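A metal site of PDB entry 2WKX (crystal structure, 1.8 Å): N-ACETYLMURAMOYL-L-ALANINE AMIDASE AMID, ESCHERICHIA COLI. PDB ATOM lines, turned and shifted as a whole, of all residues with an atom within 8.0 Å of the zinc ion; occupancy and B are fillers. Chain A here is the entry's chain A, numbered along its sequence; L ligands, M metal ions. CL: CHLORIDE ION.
A ring nitrogen (NE2) of His 151 sits at hydrogen-bond distance from the backbone carbonyl oxygen of Ala 85 (2.9 Å).
O of Asp 161 sits at hydrogen-bond distance from N of Ala 152, at 3.0 Å.
The side-chain carboxylate (OD1) of Asp 161 sits close to the backbone NH (N) of Tyr 36 (3.4 Å).
A ring nitrogen (NE2) of His 35 sits at hydrogen-bond distance from a ring nitrogen (ND1) of His 84.
The backbone NH (N) of His 35 lies within hydrogen-bond range of the backbone carbonyl oxygen (O) of Ile 103, 3.0 Å away.
The backbone NH of His 151 lies within hydrogen-bond range of the backbone carbonyl oxygen of Ile 34 (3.1 Å).
Three residues have an atom within 4 Å of the zinc ion: His 35, His 151 and Asp 161.
The side-chain carboxylate (OD1) of Asp 161 is bound to the zinc ion (2.0 Å).
The zinc ion is bound by ND1 of His 151 (2.1 Å).
A ring nitrogen (ND1) of His 35 binds the zinc ion, 2.1 Å away.
CL of the ligand is bound to the zinc ion, 2.3 Å away.
The zinc ion has four donor atoms within binding distance.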
ATOM      1  N   VAL A  33      20.523   6.864 -28.419  1.00  0.00           N
ATOM      2  CA  VAL A  33      19.380   7.786 -28.651  1.00  0.00           C
ATOM      3  C   VAL A  33      19.887   9.214 -28.668  1.00  0.00           C
ATOM      4  O   VAL A  33      20.619   9.665 -27.746  1.00  0.00           O
ATOM      5  CB  VAL A  33      18.258   7.629 -27.584  1.00  0.00           C
ATOM      6  CG1 VAL A  33      17.051   8.541 -27.938  1.00  0.00           C
ATOM      7  CG2 VAL A  33      17.805   6.133 -27.395  1.00  0.00           C
ATOM      8  N   ILE A  34      19.485   9.950 -29.710  1.00  0.00           N
ATOM      9  CA  ILE A  34      19.851  11.364 -29.862  1.00  0.00           C
ATOM     10  C   ILE A  34      18.662  12.263 -29.473  1.00  0.00           C
ATOM     11  O   ILE A  34      17.513  12.028 -29.930  1.00  0.00           O
ATOM     12  CB  ILE A  34      20.348  11.707 -31.315  1.00  0.00           C
ATOM     13  CG1 ILE A  34      21.386  10.692 -31.817  1.00  0.00           C
ATOM     14  CG2 ILE A  34      20.851  13.178 -31.448  1.00  0.00           C
ATOM     15  CD1 ILE A  34      22.710  10.602 -30.939  1.00  0.00           C
ATOM     16  N   HIS A  35      18.958  13.265 -28.662  1.00  0.00           N
ATOM     17  CA  HIS A  35      17.972  14.221 -28.134  1.00  0.00           C
ATOM     18  C   HIS A  35      18.412  15.656 -28.418  1.00  0.00           C
ATOM     19  O   HIS A  35      19.602  15.931 -28.640  1.00  0.00           O
ATOM     20  CB  HIS A  35      17.876  14.108 -26.588  1.00  0.00           C
ATOM     21  CG  HIS A  35      17.541  12.744 -26.063  1.00  0.00           C
ATOM     22  ND1 HIS A  35      16.242  12.376 -25.779  1.00  0.00           N
ATOM     23  CD2 HIS A  35      18.329  11.694 -25.723  1.00  0.00           C
ATOM     24  CE1 HIS A  35      16.240  11.125 -25.327  1.00  0.00           C
ATOM     25  NE2 HIS A  35      17.501  10.697 -25.259  1.00  0.00           N
ATOM     26  N   TYR A  36      17.459  16.587 -28.381  1.00  0.00           N
ATOM     27  CA  TYR A  36      17.819  17.980 -28.081  1.00  0.00           C
ATOM     28  C   TYR A  36      17.291  18.394 -26.705  1.00  0.00           C
ATOM     29  O   TYR A  36      16.324  17.806 -26.177  1.00  0.00           O
ATOM     30  CB  TYR A  36      17.400  19.004 -29.181  1.00  0.00           C
ATOM     31  CG  TYR A  36      15.933  19.023 -29.613  1.00  0.00           C
ATOM     32  CD1 TYR A  36      14.887  19.244 -28.704  1.00  0.00           C
ATOM     33  CD2 TYR A  36      15.613  18.867 -30.970  1.00  0.00           C
ATOM     34  CE1 TYR A  36      13.539  19.264 -29.124  1.00  0.00           C
ATOM     35  CE2 TYR A  36      14.265  18.913 -31.406  1.00  0.00           C
ATOM     36  CZ  TYR A  36      13.244  19.100 -30.469  1.00  0.00           C
ATOM     37  OH  TYR A  36      11.924  19.109 -30.868  1.00  0.00           O
ATOM     38  N   THR A  37      17.934  19.394 -26.113  1.00  0.00           N
ATOM     39  CA  THR A  37      17.609  19.799 -24.741  1.00  0.00           C
ATOM     40  C   THR A  37      16.436  20.774 -24.688  1.00  0.00           C
ATOM     41  O   THR A  37      15.787  20.924 -23.636  1.00  0.00           O
ATOM     42  CB  THR A  37      18.808  20.498 -24.046  1.00  0.00           C
ATOM     43  OG1 THR A  37      19.170  21.667 -24.802  1.00  0.00           O
ATOM     44  CG2 THR A  37      20.052  19.578 -23.936  1.00  0.00           C
ATOM     45  N   VAL A  53      15.222  13.356 -14.409  1.00  0.00           N
ATOM     46  CA  VAL A  53      15.708  13.108 -15.768  1.00  0.00           C
ATOM     47  C   VAL A  53      17.245  13.181 -15.800  1.00  0.00           C
ATOM     48  O   VAL A  53      17.859  13.851 -14.957  1.00  0.00           O
ATOM     49  CB  VAL A  53      15.031  14.104 -16.774  1.00  0.00           C
ATOM     50  CG1 VAL A  53      15.397  15.551 -16.475  1.00  0.00           C
ATOM     51  CG2 VAL A  53      15.323  13.790 -18.234  1.00  0.00           C
ATOM     52  N   HIS A  84      16.429   9.118 -19.749  1.00  0.00           N
ATOM     53  CA  HIS A  84      16.308   9.994 -20.929  1.00  0.00           C
ATOM     54  C   HIS A  84      15.198   9.592 -21.931  1.00  0.00           C
ATOM     55  O   HIS A  84      14.687  10.436 -22.687  1.00  0.00           O
ATOM     56  CB  HIS A  84      17.667  10.077 -21.663  1.00  0.00           C
ATOM     57  CG  HIS A  84      18.110   8.759 -22.223  1.00  0.00           C
ATOM     58  ND1 HIS A  84      17.943   8.415 -23.546  1.00  0.00           N
ATOM     59  CD2 HIS A  84      18.702   7.683 -21.636  1.00  0.00           C
ATOM     60  CE1 HIS A  84      18.409   7.197 -23.762  1.00  0.00           C
ATOM     61  NE2 HIS A  84      18.867   6.729 -22.612  1.00  0.00           N
ATOM     62  N   ALA A  85      14.805   8.321 -21.972  1.00  0.00           N
ATOM     63  CA  ALA A  85      13.881   7.856 -23.026  1.00  0.00           C
ATOM     64  C   ALA A  85      12.412   7.887 -22.630  1.00  0.00           C
ATOM     65  O   ALA A  85      11.546   8.000 -23.507  1.00  0.00           O
ATOM     66  CB  ALA A  85      14.267   6.461 -23.504  1.00  0.00           C
ATOM     67  N   GLY A  86      12.133   7.759 -21.325  1.00  0.00           N
ATOM     68  CA  GLY A  86      10.767   7.578 -20.812  1.00  0.00           C
ATOM     69  C   GLY A  86      10.082   6.364 -21.430  1.00  0.00           C
ATOM     70  O   GLY A  86      10.737   5.389 -21.842  1.00  0.00           O
ATOM     71  N   ILE A 103      22.336  10.659 -25.630  1.00  0.00           N
ATOM     72  CA  ILE A 103      23.152  11.867 -25.874  1.00  0.00           C
ATOM     73  C   ILE A 103      22.213  13.075 -26.022  1.00  0.00           C
ATOM     74  O   ILE A 103      21.332  13.089 -26.897  1.00  0.00           O
ATOM     75  CB  ILE A 103      24.090  11.756 -27.111  1.00  0.00           C
ATOM     76  CG1 ILE A 103      25.157  10.673 -26.895  1.00  0.00           C
ATOM     77  CG2 ILE A 103      24.766  13.129 -27.408  1.00  0.00           C
ATOM     78  CD1 ILE A 103      26.035  10.377 -28.157  1.00  0.00           C
ATOM     79  N   GLU A 104      22.406  14.071 -25.153  1.00  0.00           N
ATOM     80  CA  GLU A 104      21.650  15.330 -25.265  1.00  0.00           C
ATOM     81  C   GLU A 104      22.488  16.386 -26.014  1.00  0.00           C
ATOM     82  O   GLU A 104      23.651  16.660 -25.647  1.00  0.00           O
ATOM     83  CB  GLU A 104      21.249  15.865 -23.885  1.00  0.00           C
ATOM     84  CG  GLU A 104      20.074  15.116 -23.243  1.00  0.00           C
ATOM     85  CD  GLU A 104      18.701  15.659 -23.657  1.00  0.00           C
ATOM     86  OE1 GLU A 104      18.607  16.566 -24.509  1.00  0.00           O
ATOM     87  OE2 GLU A 104      17.670  15.177 -23.141  1.00  0.00           O
ATOM     88  N   ALA A 150      16.460   8.624 -33.235  1.00  0.00           N
ATOM     89  CA  ALA A 150      15.856   9.841 -32.665  1.00  0.00           C
ATOM     90  C   ALA A 150      15.046   9.438 -31.429  1.00  0.00           C
ATOM     91  O   ALA A 150      14.453   8.346 -31.388  1.00  0.00           O
ATOM     92  CB  ALA A 150      14.909  10.496 -33.686  1.00  0.00           C
ATOM     93  N   HIS A 151      15.000  10.299 -30.410  1.00  0.00           N
ATOM     94  CA  HIS A 151      13.975  10.109 -29.376  1.00  0.00           C
ATOM     95  C   HIS A 151      12.563   9.946 -29.990  1.00  0.00           C
ATOM     96  O   HIS A 151      11.743   9.122 -29.564  1.00  0.00           O
ATOM     97  CB  HIS A 151      14.006  11.264 -28.365  1.00  0.00           C
ATOM     98  CG  HIS A 151      13.321  10.948 -27.078  1.00  0.00           C
ATOM     99  ND1 HIS A 151      13.222  11.850 -26.057  1.00  0.00           N
ATOM    100  CD2 HIS A 151      12.679   9.822 -26.651  1.00  0.00           C
ATOM    101  CE1 HIS A 151      12.587  11.309 -25.025  1.00  0.00           C
ATOM    102  NE2 HIS A 151      12.215  10.085 -25.369  1.00  0.00           N
ATOM    103  N   ALA A 152      12.269  10.706 -31.034  1.00  0.00           N
ATOM    104  CA  ALA A 152      10.980  10.646 -31.731  1.00  0.00           C
ATOM    105  C   ALA A 152      10.725   9.257 -32.344  1.00  0.00           C
ATOM    106  O   ALA A 152       9.569   8.847 -32.446  1.00  0.00           O
ATOM    107  CB  ALA A 152      10.968  11.711 -32.856  1.00  0.00           C
ATOM    108  N   ILE A 154      11.531   6.422 -31.030  1.00  0.00           N
ATOM    109  CA  ILE A 154      11.155   5.452 -29.972  1.00  0.00           C
ATOM    110  C   ILE A 154       9.937   5.894 -29.148  1.00  0.00           C
ATOM    111  O   ILE A 154       9.355   5.103 -28.397  1.00  0.00           O
ATOM    112  CB  ILE A 154      12.358   5.118 -29.032  1.00  0.00           C
ATOM    113  CG1 ILE A 154      12.713   6.301 -28.101  1.00  0.00           C
ATOM    114  CG2 ILE A 154      13.570   4.648 -29.872  1.00  0.00           C
ATOM    115  CD1 ILE A 154      13.996   5.994 -27.198  1.00  0.00           C
ATOM    116  N   ALA A 155       9.567   7.172 -29.262  1.00  0.00           N
ATOM    117  CA  ALA A 155       8.395   7.693 -28.571  1.00  0.00           C
ATOM    118  C   ALA A 155       7.647   8.645 -29.515  1.00  0.00           C
ATOM    119  O   ALA A 155       7.529   9.843 -29.227  1.00  0.00           O
ATOM    120  CB  ALA A 155       8.859   8.438 -27.279  1.00  0.00           C
ATOM    121  N   ARG A 158       4.928  11.223 -28.493  1.00  0.00           N
ATOM    122  CA  ARG A 158       5.300  12.206 -27.441  1.00  0.00           C
ATOM    123  C   ARG A 158       6.408  13.181 -27.804  1.00  0.00           C
ATOM    124  O   ARG A 158       6.449  14.280 -27.231  1.00  0.00           O
ATOM    125  CB  ARG A 158       5.770  11.489 -26.149  1.00  0.00           C
ATOM    126  CG  ARG A 158       4.767  10.525 -25.516  1.00  0.00           C
ATOM    127  CD  ARG A 158       5.230   9.982 -24.130  1.00  0.00           C
ATOM    128  NE  ARG A 158       6.513   9.261 -24.134  1.00  0.00           N
ATOM    129  CZ  ARG A 158       7.674   9.748 -23.698  1.00  0.00           C
ATOM    130  NH1 ARG A 158       7.748  10.982 -23.199  1.00  0.00           N
ATOM    131  NH2 ARG A 158       8.786   9.018 -23.722  1.00  0.00           N
ATOM    132  N   LYS A 159       7.315  12.786 -28.694  1.00  0.00           N
ATOM    133  CA  LYS A 159       8.572  13.511 -28.919  1.00  0.00           C
ATOM    134  C   LYS A 159       8.855  13.762 -30.399  1.00  0.00           C
ATOM    135  O   LYS A 159       8.484  12.941 -31.234  1.00  0.00           O
ATOM    136  CB  LYS A 159       9.762  12.721 -28.331  1.00  0.00           C
ATOM    137  CG  LYS A 159       9.706  12.526 -26.804  1.00  0.00           C
ATOM    138  CD  LYS A 159       9.812  13.903 -26.113  1.00  0.00           C
ATOM    139  CE  LYS A 159       9.802  13.788 -24.611  1.00  0.00           C
ATOM    140  NZ  LYS A 159      10.199  15.162 -24.104  1.00  0.00           N
ATOM    141  N   ASP A 160       9.566  14.870 -30.668  1.00  0.00           N
ATOM    142  CA  ASP A 160      10.026  15.238 -32.010  1.00  0.00           C
ATOM    143  C   ASP A 160      11.557  15.197 -32.172  1.00  0.00           C
ATOM    144  O   ASP A 160      12.044  15.235 -33.298  1.00  0.00           O
ATOM    145  CB  ASP A 160       9.606  16.685 -32.349  1.00  0.00           C
ATOM    146  CG  ASP A 160       8.118  16.842 -32.649  1.00  0.00           C
ATOM    147  OD1 ASP A 160       7.347  15.848 -32.677  1.00  0.00           O
ATOM    148  OD2 ASP A 160       7.735  18.009 -32.869  1.00  0.00           O
ATOM    149  N   ASP A 161      12.286  15.179 -31.057  1.00  0.00           N
ATOM    150  CA  ASP A 161      13.750  15.387 -31.061  1.00  0.00           C
ATOM    151  C   ASP A 161      14.534  14.219 -31.667  1.00  0.00           C
ATOM    152  O   ASP A 161      14.137  13.071 -31.468  1.00  0.00           O
ATOM    153  CB  ASP A 161      14.294  15.828 -29.678  1.00  0.00           C
ATOM    154  CG  ASP A 161      13.949  14.858 -28.522  1.00  0.00           C
ATOM    155  OD1 ASP A 161      14.856  14.589 -27.701  1.00  0.00           O
ATOM    156  OD2 ASP A 161      12.791  14.410 -28.378  1.00  0.00           O
ATOM    157  N   PRO A 162      15.664  14.509 -32.368  1.00  0.00           N
ATOM    158  CA  PRO A 162      16.279  15.848 -32.592  1.00  0.00           C
ATOM    159  C   PRO A 162      15.692  16.656 -33.770  1.00  0.00           C
ATOM    160  O   PRO A 162      16.208  17.728 -34.060  1.00  0.00           O
ATOM    161  CB  PRO A 162      17.767  15.522 -32.827  1.00  0.00           C
ATOM    162  CG  PRO A 162      17.722  14.149 -33.524  1.00  0.00           C
ATOM    163  CD  PRO A 162      16.489  13.421 -32.925  1.00  0.00           C
HETATM  164 CL    CL L   1      13.590  14.741 -24.399  1.00  0.00          CL
HETATM  165 ZN    ZN M   1      14.488  13.540 -26.091  1.00  0.00          ZN
